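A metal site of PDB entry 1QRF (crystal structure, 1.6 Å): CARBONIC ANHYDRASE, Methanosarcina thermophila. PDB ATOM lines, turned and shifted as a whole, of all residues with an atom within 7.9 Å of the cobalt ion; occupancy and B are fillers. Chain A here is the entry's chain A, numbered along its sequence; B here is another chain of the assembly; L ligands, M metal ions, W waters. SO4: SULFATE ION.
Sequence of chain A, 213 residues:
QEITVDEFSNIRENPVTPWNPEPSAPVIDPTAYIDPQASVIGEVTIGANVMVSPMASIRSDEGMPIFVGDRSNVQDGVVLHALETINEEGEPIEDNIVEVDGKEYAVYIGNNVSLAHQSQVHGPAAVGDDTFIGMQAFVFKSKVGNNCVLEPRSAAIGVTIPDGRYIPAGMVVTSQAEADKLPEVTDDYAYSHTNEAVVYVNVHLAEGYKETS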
ATOM      1  N   ARG A  59      -0.573 -29.247   2.497  1.00  0.00           N
ATOM      2  CA  ARG A  59       0.854 -29.145   2.350  1.00  0.00           C
ATOM      3  C   ARG A  59       1.346 -27.728   2.576  1.00  0.00           C
ATOM      4  O   ARG A  59       1.164 -26.896   1.698  1.00  0.00           O
ATOM      5  CB  ARG A  59       1.270 -29.705   0.982  1.00  0.00           C
ATOM      6  CG  ARG A  59       2.780 -29.861   0.823  1.00  0.00           C
ATOM      7  CD  ARG A  59       3.148 -30.843  -0.300  1.00  0.00           C
ATOM      8  NE  ARG A  59       2.640 -30.424  -1.634  1.00  0.00           N
ATOM      9  CZ  ARG A  59       3.286 -29.708  -2.562  1.00  0.00           C
ATOM     10  NH1 ARG A  59       4.518 -29.232  -2.329  1.00  0.00           N
ATOM     11  NH2 ARG A  59       2.709 -29.434  -3.740  1.00  0.00           N
ATOM     12  N   ASP A  61       4.550 -26.162   2.888  1.00  0.00           N
ATOM     13  CA  ASP A  61       5.981 -26.297   2.620  1.00  0.00           C
ATOM     14  C   ASP A  61       6.540 -25.167   1.765  1.00  0.00           C
ATOM     15  O   ASP A  61       7.774 -25.049   1.552  1.00  0.00           O
ATOM     16  CB  ASP A  61       6.314 -27.634   1.949  1.00  0.00           C
ATOM     17  CG  ASP A  61       5.603 -27.883   0.615  1.00  0.00           C
ATOM     18  OD1 ASP A  61       5.876 -28.961   0.076  1.00  0.00           O
ATOM     19  OD2 ASP A  61       4.873 -27.015   0.147  1.00  0.00           O
ATOM     20  N   GLU A  62       5.649 -24.388   1.154  1.00  0.00           N
ATOM     21  CA  GLU A  62       6.040 -23.251   0.320  1.00  0.00           C
ATOM     22  C   GLU A  62       5.537 -22.039   1.087  1.00  0.00           C
ATOM     23  O   GLU A  62       6.228 -21.501   1.983  1.00  0.00           O
ATOM     24  CB  GLU A  62       5.515 -23.398  -1.098  1.00  0.00           C
ATOM     25  CG  GLU A  62       5.955 -22.296  -2.054  1.00  0.00           C
ATOM     26  CD  GLU A  62       5.326 -22.350  -3.407  1.00  0.00           C
ATOM     27  OE1 GLU A  62       4.896 -23.438  -3.846  1.00  0.00           O
ATOM     28  OE2 GLU A  62       5.213 -21.315  -4.115  1.00  0.00           O
ATOM     29  N   GLY A  63       4.315 -21.587   0.812  1.00  0.00           N
ATOM     30  CA  GLY A  63       3.635 -20.547   1.567  1.00  0.00           C
ATOM     31  C   GLY A  63       3.160 -21.191   2.889  1.00  0.00           C
ATOM     32  O   GLY A  63       2.692 -22.345   2.930  1.00  0.00           O
ATOM     33  N   VAL A  79      -7.231 -30.259  -1.770  1.00  0.00           N
ATOM     34  CA  VAL A  79      -5.821 -29.873  -1.621  1.00  0.00           C
ATOM     35  C   VAL A  79      -5.784 -28.495  -0.980  1.00  0.00           C
ATOM     36  O   VAL A  79      -6.488 -27.591  -1.440  1.00  0.00           O
ATOM     37  CB  VAL A  79      -5.115 -29.880  -2.985  1.00  0.00           C
ATOM     38  CG1 VAL A  79      -3.703 -29.246  -2.970  1.00  0.00           C
ATOM     39  CG2 VAL A  79      -4.985 -31.323  -3.483  1.00  0.00           C
ATOM     40  N   LEU A  80      -4.885 -28.256  -0.049  1.00  0.00           N
ATOM     41  CA  LEU A  80      -4.537 -26.952   0.493  1.00  0.00           C
ATOM     42  C   LEU A  80      -3.031 -26.776   0.272  1.00  0.00           C
ATOM     43  O   LEU A  80      -2.219 -27.622   0.674  1.00  0.00           O
ATOM     44  CB  LEU A  80      -4.850 -26.793   2.002  1.00  0.00           C
ATOM     45  CG  LEU A  80      -6.297 -27.029   2.415  1.00  0.00           C
ATOM     46  CD1 LEU A  80      -6.346 -26.814   3.940  1.00  0.00           C
ATOM     47  CD2 LEU A  80      -7.196 -26.056   1.660  1.00  0.00           C
ATOM     48  N   HIS A  81      -2.629 -25.738  -0.423  1.00  0.00           N
ATOM     49  CA  HIS A  81      -1.207 -25.398  -0.668  1.00  0.00           C
ATOM     50  C   HIS A  81      -1.131 -23.888  -0.851  1.00  0.00           C
ATOM     51  O   HIS A  81      -2.189 -23.256  -0.874  1.00  0.00           O
ATOM     52  CB  HIS A  81      -0.714 -26.175  -1.887  1.00  0.00           C
ATOM     53  CG  HIS A  81       0.776 -26.084  -2.079  1.00  0.00           C
ATOM     54  ND1 HIS A  81       1.452 -25.532  -3.146  1.00  0.00           N
ATOM     55  CD2 HIS A  81       1.697 -26.573  -1.218  1.00  0.00           C
ATOM     56  CE1 HIS A  81       2.777 -25.661  -2.916  1.00  0.00           C
ATOM     57  NE2 HIS A  81       2.946 -26.279  -1.756  1.00  0.00           N
ATOM     58  N   ALA A  82       0.096 -23.330  -0.913  1.00  0.00           N
ATOM     59  CA  ALA A  82       0.122 -21.857  -1.056  1.00  0.00           C
ATOM     60  C   ALA A  82       1.432 -21.349  -1.695  1.00  0.00           C
ATOM     61  O   ALA A  82       2.440 -22.021  -1.685  1.00  0.00           O
ATOM     62  CB  ALA A  82       0.036 -21.225   0.352  1.00  0.00           C
ATOM     63  N   LEU A  83       1.281 -20.189  -2.339  1.00  0.00           N
ATOM     64  CA  LEU A  83       2.444 -19.546  -2.940  1.00  0.00           C
ATOM     65  C   LEU A  83       3.438 -19.093  -1.890  1.00  0.00           C
ATOM     66  O   LEU A  83       3.075 -18.813  -0.753  1.00  0.00           O
ATOM     67  CB  LEU A  83       1.947 -18.304  -3.727  1.00  0.00           C
ATOM     68  CG  LEU A  83       1.036 -18.573  -4.932  1.00  0.00           C
ATOM     69  CD1 LEU A  83       0.605 -17.257  -5.590  1.00  0.00           C
ATOM     70  CD2 LEU A  83       1.717 -19.488  -5.927  1.00  0.00           C
ATOM     71  N   GLU A  84       4.707 -19.043  -2.290  1.00  0.00           N
ATOM     72  CA  GLU A  84       5.775 -18.669  -1.373  1.00  0.00           C
ATOM     73  C   GLU A  84       5.437 -17.373  -0.652  1.00  0.00           C
ATOM     74  O   GLU A  84       4.979 -16.355  -1.194  1.00  0.00           O
ATOM     75  CB  GLU A  84       7.095 -18.608  -2.143  1.00  0.00           C
ATOM     76  CG  GLU A  84       8.345 -18.878  -1.308  1.00  0.00           C
ATOM     77  CD  GLU A  84       9.624 -18.704  -2.117  1.00  0.00           C
ATOM     78  OE1 GLU A  84       9.626 -18.877  -3.355  1.00  0.00           O
ATOM     79  OE2 GLU A  84      10.693 -18.380  -1.536  1.00  0.00           O
ATOM     80  N   GLN A 120     -10.391 -27.230  -3.784  1.00  0.00           N
ATOM     81  CA  GLN A 120      -9.021 -26.766  -3.544  1.00  0.00           C
ATOM     82  C   GLN A 120      -9.031 -25.330  -3.087  1.00  0.00           C
ATOM     83  O   GLN A 120      -9.743 -24.504  -3.658  1.00  0.00           O
ATOM     84  CB  GLN A 120      -8.156 -26.921  -4.810  1.00  0.00           C
ATOM     85  CG  GLN A 120      -6.767 -26.343  -4.698  1.00  0.00           C
ATOM     86  CD  GLN A 120      -5.857 -26.521  -5.909  1.00  0.00           C
ATOM     87  OE1 GLN A 120      -4.793 -25.908  -5.968  1.00  0.00           O
ATOM     88  NE2 GLN A 120      -6.244 -27.372  -6.867  1.00  0.00           N
ATOM     89  N   VAL A 121      -8.207 -24.992  -2.121  1.00  0.00           N
ATOM     90  CA  VAL A 121      -8.041 -23.628  -1.625  1.00  0.00           C
ATOM     91  C   VAL A 121      -6.551 -23.389  -1.611  1.00  0.00           C
ATOM     92  O   VAL A 121      -5.780 -24.105  -0.957  1.00  0.00           O
ATOM     93  CB  VAL A 121      -8.672 -23.398  -0.264  1.00  0.00           C
ATOM     94  CG1 VAL A 121      -8.327 -21.927   0.158  1.00  0.00           C
ATOM     95  CG2 VAL A 121     -10.183 -23.575  -0.230  1.00  0.00           C
ATOM     96  N   HIS A 122      -6.103 -22.516  -2.522  1.00  0.00           N
ATOM     97  CA  HIS A 122      -4.681 -22.245  -2.693  1.00  0.00           C
ATOM     98  C   HIS A 122      -4.327 -20.833  -2.275  1.00  0.00           C
ATOM     99  O   HIS A 122      -4.939 -19.879  -2.757  1.00  0.00           O
ATOM    100  CB  HIS A 122      -4.373 -22.439  -4.217  1.00  0.00           C
ATOM    101  CG  HIS A 122      -2.900 -22.645  -4.410  1.00  0.00           C
ATOM    102  ND1 HIS A 122      -1.964 -21.639  -4.278  1.00  0.00           N
ATOM    103  CD2 HIS A 122      -2.215 -23.770  -4.705  1.00  0.00           C
ATOM    104  CE1 HIS A 122      -0.757 -22.105  -4.435  1.00  0.00           C
ATOM    105  NE2 HIS A 122      -0.861 -23.394  -4.761  1.00  0.00           N
ATOM    106  N   GLY A 123      -3.313 -20.754  -1.443  1.00  0.00           N
ATOM    107  CA  GLY A 123      -2.923 -19.423  -0.907  1.00  0.00           C
ATOM    108  C   GLY A 123      -2.269 -18.583  -1.981  1.00  0.00           C
ATOM    109  O   GLY A 123      -1.671 -19.114  -2.931  1.00  0.00           O
ATOM    110  N   PHE A 140      -8.495 -19.218  -5.081  1.00  0.00           N
ATOM    111  CA  PHE A 140      -7.084 -18.871  -5.178  1.00  0.00           C
ATOM    112  C   PHE A 140      -6.884 -17.351  -5.196  1.00  0.00           C
ATOM    113  O   PHE A 140      -7.668 -16.712  -5.876  1.00  0.00           O
ATOM    114  CB  PHE A 140      -6.588 -19.432  -6.526  1.00  0.00           C
ATOM    115  CG  PHE A 140      -5.174 -19.108  -6.892  1.00  0.00           C
ATOM    116  CD1 PHE A 140      -4.121 -19.189  -5.993  1.00  0.00           C
ATOM    117  CD2 PHE A 140      -4.889 -18.765  -8.200  1.00  0.00           C
ATOM    118  CE1 PHE A 140      -2.794 -18.924  -6.410  1.00  0.00           C
ATOM    119  CE2 PHE A 140      -3.601 -18.511  -8.627  1.00  0.00           C
ATOM    120  CZ  PHE A 140      -2.561 -18.574  -7.717  1.00  0.00           C
ATOM    121  N   GLN B  75       2.108 -32.195  -9.234  1.00  0.00           N
ATOM    122  CA  GLN B  75       1.585 -31.791  -7.938  1.00  0.00           C
ATOM    123  C   GLN B  75       0.470 -32.672  -7.406  1.00  0.00           C
ATOM    124  O   GLN B  75       0.098 -33.682  -7.977  1.00  0.00           O
ATOM    125  CB  GLN B  75       1.251 -30.266  -7.965  1.00  0.00           C
ATOM    126  CG  GLN B  75       2.515 -29.425  -8.278  1.00  0.00           C
ATOM    127  CD  GLN B  75       2.153 -27.952  -8.289  1.00  0.00           C
ATOM    128  OE1 GLN B  75       1.161 -27.496  -7.695  1.00  0.00           O
ATOM    129  NE2 GLN B  75       2.994 -27.183  -8.994  1.00  0.00           N
ATOM    130  N   ASP B  76      -0.040 -32.257  -6.231  1.00  0.00           N
ATOM    131  CA  ASP B  76      -0.916 -33.126  -5.449  1.00  0.00           C
ATOM    132  C   ASP B  76      -2.177 -33.461  -6.208  1.00  0.00           C
ATOM    133  O   ASP B  76      -2.826 -32.605  -6.790  1.00  0.00           O
ATOM    134  CB  ASP B  76      -1.357 -32.469  -4.120  1.00  0.00           C
ATOM    135  CG  ASP B  76      -0.260 -31.735  -3.371  1.00  0.00           C
ATOM    136  OD1 ASP B  76       0.289 -30.772  -3.947  1.00  0.00           O
ATOM    137  OD2 ASP B  76       0.077 -32.132  -2.226  1.00  0.00           O
ATOM    138  N   ALA B 116       0.086 -28.353 -12.026  1.00  0.00           N
ATOM    139  CA  ALA B 116      -0.375 -27.918 -10.700  1.00  0.00           C
ATOM    140  C   ALA B 116      -1.469 -28.795 -10.121  1.00  0.00           C
ATOM    141  O   ALA B 116      -2.093 -29.615 -10.792  1.00  0.00           O
ATOM    142  CB  ALA B 116      -0.751 -26.463 -10.799  1.00  0.00           C
ATOM    143  N   HIS B 117      -1.712 -28.587  -8.847  1.00  0.00           N
ATOM    144  CA  HIS B 117      -2.604 -29.416  -8.057  1.00  0.00           C
ATOM    145  C   HIS B 117      -3.908 -29.785  -8.747  1.00  0.00           C
ATOM    146  O   HIS B 117      -4.623 -28.856  -9.209  1.00  0.00           O
ATOM    147  CB  HIS B 117      -2.912 -28.783  -6.728  1.00  0.00           C
ATOM    148  CG  HIS B 117      -1.781 -28.128  -6.038  1.00  0.00           C
ATOM    149  ND1 HIS B 117      -0.846 -28.729  -5.215  1.00  0.00           N
ATOM    150  CD2 HIS B 117      -1.580 -26.795  -6.069  1.00  0.00           C
ATOM    151  CE1 HIS B 117      -0.061 -27.762  -4.787  1.00  0.00           C
ATOM    152  NE2 HIS B 117      -0.439 -26.549  -5.306  1.00  0.00           N
ATOM    153  N   PHE B 132       3.170 -23.920 -17.838  1.00  0.00           N
ATOM    154  CA  PHE B 132       2.449 -24.080 -16.559  1.00  0.00           C
ATOM    155  C   PHE B 132       1.085 -24.661 -16.866  1.00  0.00           C
ATOM    156  O   PHE B 132       0.306 -24.044 -17.586  1.00  0.00           O
ATOM    157  CB  PHE B 132       2.361 -22.759 -15.834  1.00  0.00           C
ATOM    158  CG  PHE B 132       1.627 -22.712 -14.522  1.00  0.00           C
ATOM    159  CD1 PHE B 132       2.211 -23.164 -13.349  1.00  0.00           C
ATOM    160  CD2 PHE B 132       0.323 -22.281 -14.460  1.00  0.00           C
ATOM    161  CE1 PHE B 132       1.502 -23.125 -12.168  1.00  0.00           C
ATOM    162  CE2 PHE B 132      -0.418 -22.234 -13.292  1.00  0.00           C
ATOM    163  CZ  PHE B 132       0.202 -22.684 -12.108  1.00  0.00           C
ATOM    164  N   MET B 135      -3.919 -25.181 -11.775  1.00  0.00           N
ATOM    165  CA  MET B 135      -4.735 -25.986 -10.872  1.00  0.00           C
ATOM    166  C   MET B 135      -6.035 -26.430 -11.510  1.00  0.00           C
ATOM    167  O   MET B 135      -6.758 -25.619 -12.107  1.00  0.00           O
ATOM    168  CB  MET B 135      -5.007 -25.166  -9.613  1.00  0.00           C
ATOM    169  CG  MET B 135      -3.815 -24.666  -8.810  1.00  0.00           C
ATOM    170  SD  MET B 135      -3.233 -23.064  -9.473  1.00  0.00           S
ATOM    171  CE  MET B 135      -2.002 -22.573  -8.292  1.00  0.00           C
ATOM    172  N   VAL B 198       7.555 -21.280 -10.027  1.00  0.00           N
ATOM    173  CA  VAL B 198       7.142 -22.599  -9.609  1.00  0.00           C
ATOM    174  C   VAL B 198       8.208 -23.663  -9.751  1.00  0.00           C
ATOM    175  O   VAL B 198       8.422 -24.567  -8.902  1.00  0.00           O
ATOM    176  CB  VAL B 198       5.848 -23.020 -10.367  1.00  0.00           C
ATOM    177  CG1 VAL B 198       5.386 -24.394  -9.979  1.00  0.00           C
ATOM    178  CG2 VAL B 198       4.767 -21.965 -10.062  1.00  0.00           C
ATOM    179  N   VAL B 201      10.919 -23.157  -7.138  1.00  0.00           N
ATOM    180  CA  VAL B 201      10.435 -23.657  -5.816  1.00  0.00           C
ATOM    181  C   VAL B 201      10.457 -25.149  -5.776  1.00  0.00           C
ATOM    182  O   VAL B 201      10.908 -25.845  -4.854  1.00  0.00           O
ATOM    183  CB  VAL B 201       8.999 -23.133  -5.556  1.00  0.00           C
ATOM    184  CG1 VAL B 201       8.408 -23.812  -4.314  1.00  0.00           C
ATOM    185  CG2 VAL B 201       9.065 -21.631  -5.390  1.00  0.00           C
ATOM    186  N   ASN B 202       9.891 -25.812  -6.790  1.00  0.00           N
ATOM    187  CA  ASN B 202       9.745 -27.246  -6.831  1.00  0.00           C
ATOM    188  C   ASN B 202      11.015 -28.041  -6.963  1.00  0.00           C
ATOM    189  O   ASN B 202      11.183 -29.085  -6.352  1.00  0.00           O
ATOM    190  CB  ASN B 202       8.705 -27.712  -7.867  1.00  0.00           C
ATOM    191  CG  ASN B 202       7.274 -27.545  -7.333  1.00  0.00           C
ATOM    192  OD1 ASN B 202       6.764 -28.546  -6.814  1.00  0.00           O
ATOM    193  ND2 ASN B 202       6.726 -26.353  -7.461  1.00  0.00           N
ATOM    194  N   LEU B 205      12.141 -27.930  -3.448  1.00  0.00           N
ATOM    195  CA  LEU B 205      11.371 -28.841  -2.604  1.00  0.00           C
ATOM    196  C   LEU B 205      11.773 -30.286  -2.827  1.00  0.00           C
ATOM    197  O   LEU B 205      11.915 -31.088  -1.882  1.00  0.00           O
ATOM    198  CB  LEU B 205       9.870 -28.655  -2.891  1.00  0.00           C
ATOM    199  CG  LEU B 205       9.199 -27.465  -2.265  1.00  0.00           C
ATOM    200  CD1 LEU B 205       7.729 -27.406  -2.760  1.00  0.00           C
ATOM    201  CD2 LEU B 205       9.190 -27.552  -0.724  1.00  0.00           C
HETATM  202  S   SO4 L   1       3.199 -24.008  -6.389  1.00  0.00           S
HETATM  203  O1  SO4 L   1       4.663 -23.801  -6.279  1.00  0.00           O
HETATM  204  O2  SO4 L   1       2.631 -23.664  -7.716  1.00  0.00           O
HETATM  205  O3  SO4 L   1       3.006 -25.510  -6.155  1.00  0.00           O
HETATM  206  O4  SO4 L   1       2.522 -23.197  -5.284  1.00  0.00           O
HETATM  207 CO    CO M   1       0.713 -24.792  -4.993  1.00  0.00          CO
HETATM  208  O   HOH W   1       0.373 -24.848  -7.247  1.00  0.00           O
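A ring nitrogen (NE2) of His 81 lies within hydrogen-bond range of the guanidinium group (NH1) of Arg 59 (3.4 Å).
The backbone carbonyl oxygen (O) of His 81 sits at hydrogen-bond distance from the backbone NH (N) of Gly 123.
NE2 of His 81 lies within hydrogen-bond range of OD2 of Asp 61, at 2.8 Å.
The backbone carbonyl oxygen (O) of His 117 of chain B sits at hydrogen-bond distance from the side-chain amide nitrogen (NE2) of Gln 120, 3.2 Å away.
The backbone NH (N) of His 117 of chain B sits close to the side-chain amide oxygen (OE1) of Gln 75 of chain B (3.3 Å).
The side-chain carboxylate (OD1) of Asp 76 of chain B is in hydrogen-bond range of a ring nitrogen (ND1) of His 117 of chain B (2.7 Å).
Gln 75 of chain B touches the cobalt ion.
Four residues have an atom within 4 Å of the cobalt ion: His 81, His 122, Gln 75 of chain B and His 117 of chain B.
The cobalt ion is bound by a ring nitrogen (NE2) of His 122, 2.1 Å away.
A ring nitrogen (ND1) of His 81 binds the cobalt ion (2.1 Å).
The cobalt ion is bound by NE2 of His 117 of chain B, at 2.1 Å.
Water W1 is bound to the cobalt ion (2.3 Å).
O4 of the ligand is bound to the cobalt ion (2.4 Å).
The cobalt ion has five donor atoms within binding distance.
Slightly farther from the cobalt ion lies O3 of the ligand (2.7 Å).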
